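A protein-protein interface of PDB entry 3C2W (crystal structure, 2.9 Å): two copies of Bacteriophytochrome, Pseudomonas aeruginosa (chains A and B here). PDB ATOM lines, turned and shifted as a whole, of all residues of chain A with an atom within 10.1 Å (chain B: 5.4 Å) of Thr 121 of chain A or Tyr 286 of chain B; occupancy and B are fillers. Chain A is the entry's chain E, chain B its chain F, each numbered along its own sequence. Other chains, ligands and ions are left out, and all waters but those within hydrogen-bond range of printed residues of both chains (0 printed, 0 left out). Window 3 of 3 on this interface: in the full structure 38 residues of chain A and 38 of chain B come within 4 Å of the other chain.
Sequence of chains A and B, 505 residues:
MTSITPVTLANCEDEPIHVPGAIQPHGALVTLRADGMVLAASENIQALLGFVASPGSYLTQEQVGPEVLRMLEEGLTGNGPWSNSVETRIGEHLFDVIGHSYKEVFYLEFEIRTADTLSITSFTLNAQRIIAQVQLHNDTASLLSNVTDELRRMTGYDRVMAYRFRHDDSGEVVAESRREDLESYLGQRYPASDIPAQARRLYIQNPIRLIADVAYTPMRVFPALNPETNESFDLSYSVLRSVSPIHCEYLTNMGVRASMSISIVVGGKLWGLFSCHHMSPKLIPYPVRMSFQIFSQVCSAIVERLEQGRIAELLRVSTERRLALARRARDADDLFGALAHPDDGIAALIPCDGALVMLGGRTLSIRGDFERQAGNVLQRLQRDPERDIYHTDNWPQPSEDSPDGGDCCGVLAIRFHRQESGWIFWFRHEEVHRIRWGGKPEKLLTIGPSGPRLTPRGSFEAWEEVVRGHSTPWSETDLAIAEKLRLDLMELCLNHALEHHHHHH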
ATOM      1  N   LEU A 118      30.015  10.574 -36.657  1.00  0.00           N
ATOM      2  CA  LEU A 118      29.167  10.928 -35.525  1.00  0.00           C
ATOM      3  C   LEU A 118      29.220   9.887 -34.406  1.00  0.00           C
ATOM      4  O   LEU A 118      29.778   8.801 -34.574  1.00  0.00           O
ATOM      5  CB  LEU A 118      27.722  11.122 -35.985  1.00  0.00           C
ATOM      6  CG  LEU A 118      27.383  12.512 -36.523  1.00  0.00           C
ATOM      7  CD1 LEU A 118      25.889  12.633 -36.785  1.00  0.00           C
ATOM      8  CD2 LEU A 118      27.855  13.591 -35.555  1.00  0.00           C
ATOM      9  N   SER A 119      28.631  10.230 -33.264  1.00  0.00           N
ATOM     10  CA  SER A 119      28.555   9.316 -32.131  1.00  0.00           C
ATOM     11  C   SER A 119      27.228   8.565 -32.172  1.00  0.00           C
ATOM     12  O   SER A 119      26.163   9.179 -32.240  1.00  0.00           O
ATOM     13  CB  SER A 119      28.704  10.078 -30.812  1.00  0.00           C
ATOM     14  OG  SER A 119      29.994  10.655 -30.685  1.00  0.00           O
ATOM     15  N   ILE A 120      27.292   7.238 -32.125  1.00  0.00           N
ATOM     16  CA  ILE A 120      26.101   6.411 -32.295  1.00  0.00           C
ATOM     17  C   ILE A 120      25.157   6.433 -31.099  1.00  0.00           C
ATOM     18  O   ILE A 120      23.944   6.519 -31.271  1.00  0.00           O
ATOM     19  CB  ILE A 120      26.471   4.952 -32.588  1.00  0.00           C
ATOM     20  CG1 ILE A 120      27.156   4.846 -33.949  1.00  0.00           C
ATOM     21  CG2 ILE A 120      25.233   4.075 -32.540  1.00  0.00           C
ATOM     22  CD1 ILE A 120      27.702   3.471 -34.243  1.00  0.00           C
ATOM     23  N   THR A 121      25.709   6.337 -29.893  1.00  0.00           N
ATOM     24  CA  THR A 121      24.883   6.386 -28.696  1.00  0.00           C
ATOM     25  C   THR A 121      24.124   7.712 -28.630  1.00  0.00           C
ATOM     26  O   THR A 121      23.026   7.781 -28.080  1.00  0.00           O
ATOM     27  CB  THR A 121      25.709   6.182 -27.409  1.00  0.00           C
ATOM     28  OG1 THR A 121      26.568   5.044 -27.557  1.00  0.00           O
ATOM     29  CG2 THR A 121      24.791   5.961 -26.217  1.00  0.00           C
ATOM     30  N   SER A 122      24.717   8.757 -29.206  1.00  0.00           N
ATOM     31  CA  SER A 122      24.112  10.091 -29.236  1.00  0.00           C
ATOM     32  C   SER A 122      23.030  10.206 -30.312  1.00  0.00           C
ATOM     33  O   SER A 122      22.486  11.287 -30.548  1.00  0.00           O
ATOM     34  CB  SER A 122      25.189  11.155 -29.476  1.00  0.00           C
ATOM     35  OG  SER A 122      26.276  10.994 -28.580  1.00  0.00           O
ATOM     36  N   PHE A 123      22.741   9.091 -30.974  1.00  0.00           N
ATOM     37  CA  PHE A 123      21.659   9.023 -31.947  1.00  0.00           C
ATOM     38  C   PHE A 123      20.630   7.997 -31.494  1.00  0.00           C
ATOM     39  O   PHE A 123      19.432   8.145 -31.741  1.00  0.00           O
ATOM     40  CB  PHE A 123      22.191   8.641 -33.329  1.00  0.00           C
ATOM     41  CG  PHE A 123      21.144   8.060 -34.238  1.00  0.00           C
ATOM     42  CD1 PHE A 123      20.505   8.842 -35.181  1.00  0.00           C
ATOM     43  CD2 PHE A 123      20.792   6.726 -34.141  1.00  0.00           C
ATOM     44  CE1 PHE A 123      19.535   8.299 -36.005  1.00  0.00           C
ATOM     45  CE2 PHE A 123      19.827   6.179 -34.964  1.00  0.00           C
ATOM     46  CZ  PHE A 123      19.198   6.964 -35.900  1.00  0.00           C
ATOM     47  N   THR A 124      21.109   6.940 -30.850  1.00  0.00           N
ATOM     48  CA  THR A 124      20.213   5.954 -30.263  1.00  0.00           C
ATOM     49  C   THR A 124      19.554   6.563 -29.039  1.00  0.00           C
ATOM     50  O   THR A 124      18.610   6.004 -28.482  1.00  0.00           O
ATOM     51  CB  THR A 124      20.964   4.690 -29.810  1.00  0.00           C
ATOM     52  OG1 THR A 124      21.992   4.377 -30.756  1.00  0.00           O
ATOM     53  CG2 THR A 124      19.999   3.513 -29.693  1.00  0.00           C
ATOM     54  N   LEU A 125      20.067   7.714 -28.617  1.00  0.00           N
ATOM     55  CA  LEU A 125      19.566   8.369 -27.416  1.00  0.00           C
ATOM     56  C   LEU A 125      18.377   9.266 -27.739  1.00  0.00           C
ATOM     57  O   LEU A 125      17.335   9.187 -27.080  1.00  0.00           O
ATOM     58  CB  LEU A 125      20.674   9.168 -26.725  1.00  0.00           C
ATOM     59  CG  LEU A 125      20.573   9.296 -25.202  1.00  0.00           C
ATOM     60  CD1 LEU A 125      21.898   9.747 -24.598  1.00  0.00           C
ATOM     61  CD2 LEU A 125      19.449  10.249 -24.802  1.00  0.00           C
ATOM     62  N   ASN A 126      18.528  10.117 -28.749  1.00  0.00           N
ATOM     63  CA  ASN A 126      17.435  10.990 -29.150  1.00  0.00           C
ATOM     64  C   ASN A 126      16.556  10.385 -30.242  1.00  0.00           C
ATOM     65  O   ASN A 126      15.882  11.102 -30.981  1.00  0.00           O
ATOM     66  CB  ASN A 126      17.944  12.387 -29.539  1.00  0.00           C
ATOM     67  CG  ASN A 126      18.638  12.411 -30.888  1.00  0.00           C
ATOM     68  OD1 ASN A 126      18.935  11.368 -31.468  1.00  0.00           O
ATOM     69  ND2 ASN A 126      18.913  13.616 -31.390  1.00  0.00           N
ATOM     70  N   ALA A 127      16.577   9.060 -30.335  1.00  0.00           N
ATOM     71  CA  ALA A 127      15.570   8.351 -31.100  1.00  0.00           C
ATOM     72  C   ALA A 127      14.455   7.998 -30.128  1.00  0.00           C
ATOM     73  O   ALA A 127      13.361   7.611 -30.532  1.00  0.00           O
ATOM     74  CB  ALA A 127      16.157   7.104 -31.740  1.00  0.00           C
ATOM     75  N   GLN A 128      14.746   8.146 -28.838  1.00  0.00           N
ATOM     76  CA  GLN A 128      13.743   7.999 -27.785  1.00  0.00           C
ATOM     77  C   GLN A 128      13.012   9.316 -27.548  1.00  0.00           C
ATOM     78  O   GLN A 128      11.866   9.330 -27.101  1.00  0.00           O
ATOM     79  CB  GLN A 128      14.387   7.522 -26.478  1.00  0.00           C
ATOM     80  CG  GLN A 128      14.212   6.039 -26.206  1.00  0.00           C
ATOM     81  CD  GLN A 128      12.824   5.696 -25.683  1.00  0.00           C
ATOM     82  OE1 GLN A 128      12.302   6.370 -24.792  1.00  0.00           O
ATOM     83  NE2 GLN A 128      12.220   4.646 -26.235  1.00  0.00           N
ATOM     84  N   ARG A 129      13.685  10.425 -27.837  1.00  0.00           N
ATOM     85  CA  ARG A 129      13.052  11.732 -27.764  1.00  0.00           C
ATOM     86  C   ARG A 129      11.939  11.773 -28.800  1.00  0.00           C
ATOM     87  O   ARG A 129      11.050  12.613 -28.736  1.00  0.00           O
ATOM     88  CB  ARG A 129      14.069  12.844 -28.033  1.00  0.00           C
ATOM     89  CG  ARG A 129      13.502  14.266 -28.048  1.00  0.00           C
ATOM     90  CD  ARG A 129      13.333  14.821 -26.638  1.00  0.00           C
ATOM     91  NE  ARG A 129      13.547  16.265 -26.570  1.00  0.00           N
ATOM     92  CZ  ARG A 129      12.633  17.169 -26.908  1.00  0.00           C
ATOM     93  NH1 ARG A 129      11.443  16.779 -27.349  1.00  0.00           N
ATOM     94  NH2 ARG A 129      12.911  18.463 -26.809  1.00  0.00           N
ATOM     95  N   MET A 154      19.152  17.634 -35.520  1.00  0.00           N
ATOM     96  CA  MET A 154      20.126  16.581 -35.813  1.00  0.00           C
ATOM     97  C   MET A 154      21.124  16.966 -36.907  1.00  0.00           C
ATOM     98  O   MET A 154      22.324  16.709 -36.785  1.00  0.00           O
ATOM     99  CB  MET A 154      19.406  15.286 -36.217  1.00  0.00           C
ATOM    100  CG  MET A 154      19.330  14.228 -35.121  1.00  0.00           C
ATOM    101  SD  MET A 154      20.400  12.797 -35.409  1.00  0.00           S
ATOM    102  CE  MET A 154      22.039  13.520 -35.323  1.00  0.00           C
ATOM    103  N   SER A 291      22.262   6.334 -41.317  1.00  0.00           N
ATOM    104  CA  SER A 291      21.691   6.518 -39.993  1.00  0.00           C
ATOM    105  C   SER A 291      20.279   7.096 -40.095  1.00  0.00           C
ATOM    106  O   SER A 291      19.378   6.671 -39.371  1.00  0.00           O
ATOM    107  CB  SER A 291      22.574   7.431 -39.143  1.00  0.00           C
ATOM    108  OG  SER A 291      21.810   8.073 -38.132  1.00  0.00           O
ATOM    109  N   SER B  83      25.175   9.921 -21.244  1.00  0.00           N
ATOM    110  CA  SER B  83      25.304   8.665 -21.972  1.00  0.00           C
ATOM    111  C   SER B  83      26.096   8.838 -23.268  1.00  0.00           C
ATOM    112  O   SER B  83      25.814   9.742 -24.057  1.00  0.00           O
ATOM    113  CB  SER B  83      23.916   8.089 -22.266  1.00  0.00           C
ATOM    114  OG  SER B  83      23.976   6.706 -22.557  1.00  0.00           O
ATOM    115  N   ASN B  84      27.092   7.978 -23.483  1.00  0.00           N
ATOM    116  CA  ASN B  84      27.885   8.024 -24.711  1.00  0.00           C
ATOM    117  C   ASN B  84      28.839   6.833 -24.854  1.00  0.00           C
ATOM    118  O   ASN B  84      28.996   6.043 -23.923  1.00  0.00           O
ATOM    119  CB  ASN B  84      28.660   9.342 -24.790  1.00  0.00           C
ATOM    120  CG  ASN B  84      28.769   9.872 -26.213  1.00  0.00           C
ATOM    121  OD1 ASN B  84      29.263  10.976 -26.438  1.00  0.00           O
ATOM    122  ND2 ASN B  84      28.309   9.085 -27.178  1.00  0.00           N
ATOM    123  N   SER B  85      29.471   6.711 -26.020  1.00  0.00           N
ATOM    124  CA  SER B  85      30.385   5.601 -26.291  1.00  0.00           C
ATOM    125  C   SER B  85      31.487   5.988 -27.267  1.00  0.00           C
ATOM    126  O   SER B  85      31.308   6.886 -28.087  1.00  0.00           O
ATOM    127  CB  SER B  85      29.616   4.412 -26.864  1.00  0.00           C
ATOM    128  OG  SER B  85      29.155   4.692 -28.177  1.00  0.00           O
ATOM    129  N   ASP B  96      35.390  -0.767 -26.609  1.00  0.00           N
ATOM    130  CA  ASP B  96      34.240   0.119 -26.559  1.00  0.00           C
ATOM    131  C   ASP B  96      34.235   0.798 -25.205  1.00  0.00           C
ATOM    132  O   ASP B  96      34.159   0.131 -24.174  1.00  0.00           O
ATOM    133  CB  ASP B  96      32.944  -0.677 -26.698  1.00  0.00           C
ATOM    134  CG  ASP B  96      32.603  -1.003 -28.128  1.00  0.00           C
ATOM    135  OD1 ASP B  96      32.471  -0.061 -28.934  1.00  0.00           O
ATOM    136  OD2 ASP B  96      32.451  -2.202 -28.430  1.00  0.00           O
ATOM    137  N   ILE B  98      32.117   2.464 -22.926  1.00  0.00           N
ATOM    138  CA  ILE B  98      30.683   2.650 -22.733  1.00  0.00           C
ATOM    139  C   ILE B  98      30.352   3.244 -21.367  1.00  0.00           C
ATOM    140  O   ILE B  98      30.167   2.519 -20.388  1.00  0.00           O
ATOM    141  CB  ILE B  98      29.930   1.332 -22.952  1.00  0.00           C
ATOM    142  CG1 ILE B  98      30.645   0.184 -22.235  1.00  0.00           C
ATOM    143  CG2 ILE B  98      29.852   1.027 -24.431  1.00  0.00           C
ATOM    144  CD1 ILE B  98      30.239  -1.195 -22.710  1.00  0.00           C
ATOM    145  N   GLU B 111      34.645  -2.912 -23.065  1.00  0.00           N
ATOM    146  CA  GLU B 111      34.415  -4.201 -23.700  1.00  0.00           C
ATOM    147  C   GLU B 111      35.344  -4.401 -24.899  1.00  0.00           C
ATOM    148  O   GLU B 111      35.606  -3.467 -25.660  1.00  0.00           O
ATOM    149  CB  GLU B 111      32.950  -4.320 -24.129  1.00  0.00           C
ATOM    150  CG  GLU B 111      32.338  -5.695 -23.892  1.00  0.00           C
ATOM    151  CD  GLU B 111      30.850  -5.732 -24.198  1.00  0.00           C
ATOM    152  OE1 GLU B 111      30.096  -6.365 -23.431  1.00  0.00           O
ATOM    153  OE2 GLU B 111      30.440  -5.131 -25.210  1.00  0.00           O
ATOM    154  N   ILE B 284      27.790 -10.443 -27.614  1.00  0.00           N
ATOM    155  CA  ILE B 284      27.437  -9.587 -28.740  1.00  0.00           C
ATOM    156  C   ILE B 284      28.114  -8.220 -28.634  1.00  0.00           C
ATOM    157  O   ILE B 284      28.040  -7.564 -27.594  1.00  0.00           O
ATOM    158  CB  ILE B 284      25.909  -9.393 -28.868  1.00  0.00           C
ATOM    159  CG1 ILE B 284      25.276 -10.552 -29.646  1.00  0.00           C
ATOM    160  CG2 ILE B 284      25.611  -8.094 -29.591  1.00  0.00           C
ATOM    161  CD1 ILE B 284      24.937 -11.750 -28.811  1.00  0.00           C
ATOM    162  N   PRO B 285      28.782  -7.803 -29.719  1.00  0.00           N
ATOM    163  CA  PRO B 285      29.476  -6.516 -29.815  1.00  0.00           C
ATOM    164  C   PRO B 285      28.543  -5.377 -29.435  1.00  0.00           C
ATOM    165  O   PRO B 285      27.337  -5.478 -29.659  1.00  0.00           O
ATOM    166  CB  PRO B 285      29.840  -6.432 -31.293  1.00  0.00           C
ATOM    167  CG  PRO B 285      29.954  -7.848 -31.731  1.00  0.00           C
ATOM    168  CD  PRO B 285      28.927  -8.607 -30.945  1.00  0.00           C
ATOM    169  N   TYR B 286      29.098  -4.310 -28.873  1.00  0.00           N
ATOM    170  CA  TYR B 286      28.288  -3.190 -28.407  1.00  0.00           C
ATOM    171  C   TYR B 286      27.503  -2.487 -29.522  1.00  0.00           C
ATOM    172  O   TYR B 286      26.325  -2.165 -29.341  1.00  0.00           O
ATOM    173  CB  TYR B 286      29.136  -2.178 -27.633  1.00  0.00           C
ATOM    174  CG  TYR B 286      28.363  -0.973 -27.151  1.00  0.00           C
ATOM    175  CD1 TYR B 286      27.701  -0.996 -25.931  1.00  0.00           C
ATOM    176  CD2 TYR B 286      28.296   0.186 -27.916  1.00  0.00           C
ATOM    177  CE1 TYR B 286      26.996   0.105 -25.481  1.00  0.00           C
ATOM    178  CE2 TYR B 286      27.584   1.288 -27.479  1.00  0.00           C
ATOM    179  CZ  TYR B 286      26.941   1.247 -26.261  1.00  0.00           C
ATOM    180  OH  TYR B 286      26.239   2.353 -25.832  1.00  0.00           O
ATOM    181  N   PRO B 287      28.148  -2.244 -30.678  1.00  0.00           N
ATOM    182  CA  PRO B 287      27.442  -1.587 -31.787  1.00  0.00           C
ATOM    183  C   PRO B 287      26.254  -2.409 -32.287  1.00  0.00           C
ATOM    184  O   PRO B 287      25.389  -1.878 -32.983  1.00  0.00           O
ATOM    185  CB  PRO B 287      28.511  -1.504 -32.883  1.00  0.00           C
ATOM    186  CG  PRO B 287      29.806  -1.550 -32.150  1.00  0.00           C
ATOM    187  CD  PRO B 287      29.574  -2.447 -30.979  1.00  0.00           C
ATOM    188  N   VAL B 288      26.223  -3.694 -31.942  1.00  0.00           N
ATOM    189  CA  VAL B 288      25.129  -4.578 -32.339  1.00  0.00           C
ATOM    190  C   VAL B 288      24.067  -4.686 -31.236  1.00  0.00           C
ATOM    191  O   VAL B 288      22.906  -4.994 -31.508  1.00  0.00           O
ATOM    192  CB  VAL B 288      25.644  -5.987 -32.734  1.00  0.00           C
ATOM    193  CG1 VAL B 288      24.484  -6.935 -32.988  1.00  0.00           C
ATOM    194  CG2 VAL B 288      26.538  -5.908 -33.958  1.00  0.00           C
ATOM    195  N   ARG B 289      24.470  -4.425 -29.995  1.00  0.00           N
ATOM    196  CA  ARG B 289      23.526  -4.388 -28.880  1.00  0.00           C
ATOM    197  C   ARG B 289      22.699  -3.104 -28.895  1.00  0.00           C
ATOM    198  O   ARG B 289      21.571  -3.076 -28.396  1.00  0.00           O
ATOM    199  CB  ARG B 289      24.242  -4.527 -27.531  1.00  0.00           C
ATOM    200  CG  ARG B 289      24.964  -5.858 -27.329  1.00  0.00           C
ATOM    201  CD  ARG B 289      25.114  -6.185 -25.847  1.00  0.00           C
ATOM    202  NE  ARG B 289      25.458  -5.004 -25.061  1.00  0.00           N
ATOM    203  CZ  ARG B 289      26.676  -4.727 -24.609  1.00  0.00           C
ATOM    204  NH1 ARG B 289      27.684  -5.551 -24.861  1.00  0.00           N
ATOM    205  NH2 ARG B 289      26.883  -3.618 -23.912  1.00  0.00           N
ATOM    206  N   MET B 290      23.268  -2.042 -29.459  1.00  0.00           N
ATOM    207  CA  MET B 290      22.552  -0.778 -29.590  1.00  0.00           C
ATOM    208  C   MET B 290      21.670  -0.838 -30.827  1.00  0.00           C
ATOM    209  O   MET B 290      20.673  -0.124 -30.930  1.00  0.00           O
ATOM    210  CB  MET B 290      23.523   0.400 -29.691  1.00  0.00           C
ATOM    211  CG  MET B 290      24.469   0.547 -28.519  1.00  0.00           C
ATOM    212  SD  MET B 290      23.688   1.117 -26.994  1.00  0.00           S
ATOM    213  CE  MET B 290      23.391   2.840 -27.380  1.00  0.00           C
ATOM    214  N   SER B 291      22.051  -1.701 -31.764  1.00  0.00           N
ATOM    215  CA  SER B 291      21.240  -1.956 -32.948  1.00  0.00           C
ATOM    216  C   SER B 291      20.002  -2.744 -32.550  1.00  0.00           C
ATOM    217  O   SER B 291      19.042  -2.852 -33.315  1.00  0.00           O
ATOM    218  CB  SER B 291      22.033  -2.733 -33.997  1.00  0.00           C
ATOM    219  OG  SER B 291      21.312  -2.816 -35.214  1.00  0.00           O
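OG of Ser 122 of chain A is in hydrogen-bond range of ND2 of Asn 84 of chain B (3.1 Å).
OG of Ser 85 of chain B lies within hydrogen-bond range of OG1 of Thr 121 of chain A, at 2.7 Å.
The side-chain hydroxyl (OH) of Tyr 286 of chain B is in hydrogen-bond range of the side-chain hydroxyl (OG1) of Thr 121 of chain A (3.2 Å).
O of Ile 120 of chain A lies within hydrogen-bond range of OG1 of Thr 124 of chain A, at 2.9 Å.
The side-chain hydroxyl (OH) of Tyr 286 of chain B sits at hydrogen-bond distance from the side-chain sulfur (SD) of Met 290 of chain B, at 3.1 Å.
Among the printed residues, pairs that only touch across the chains: Leu 125 of chain A with Ser 83 of chain B (3.5 Å), Thr 121 of chain A with Met 290 of chain B (3.6 Å), Ser 119 of chain A with Asn 84 of chain B (3.8 Å), Thr 121 of chain A with Ser 83 of chain B (3.8 Å), Thr 124 of chain A with Met 290 of chain B (3.9 Å) and Thr 121 of chain A with Asn 84 of chain B (3.9 Å).
Thr 121 of chain A touches just these residues of chain B: Ser 83, Asn 84, Ser 85, Tyr 286 and Met 290.
Printed residues of chain B within 4 Å of Ser 122 of chain A: Asn 84.
Printed residues of chain B within 4 Å of Leu 125 of chain A: Ser 83.
Of chain A, only Thr 121 comes within 4 Å of Ser 85 of chain B.
No residue of chain A comes within 4 Å of Pro 285 of chain B.
Tyr 286 of chain B touches just one residue of chain A: Thr 121.
No residue of chain A comes within 4 Å of Pro 287 of chain B.
The nearest residue of chain A that does not touch Tyr 286 of chain B is Ile 120 of chain A (6.2 Å).
The nearest printed residue of chain A that does not touch Met 290 of chain B is Ile 120 of chain A (5.0 Å).
Hydrophobic or aromatic side chains of chain A that line the printed part of chain B: Leu 125.
Of the 14 printed residues of chain B, 5 touch a printed residue of chain A.
Printed residues of chain B that touch a printed residue of chain A: Ser 83, Asn 84, Ser 85, Tyr 286 and Met 290.
Hydrophobic or aromatic side chains of chain B that line the printed part of chain A: Tyr 286 and Met 290.
Among the printed residues, 9 pairs touch across the chains.
Position printed for both chains: 291.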
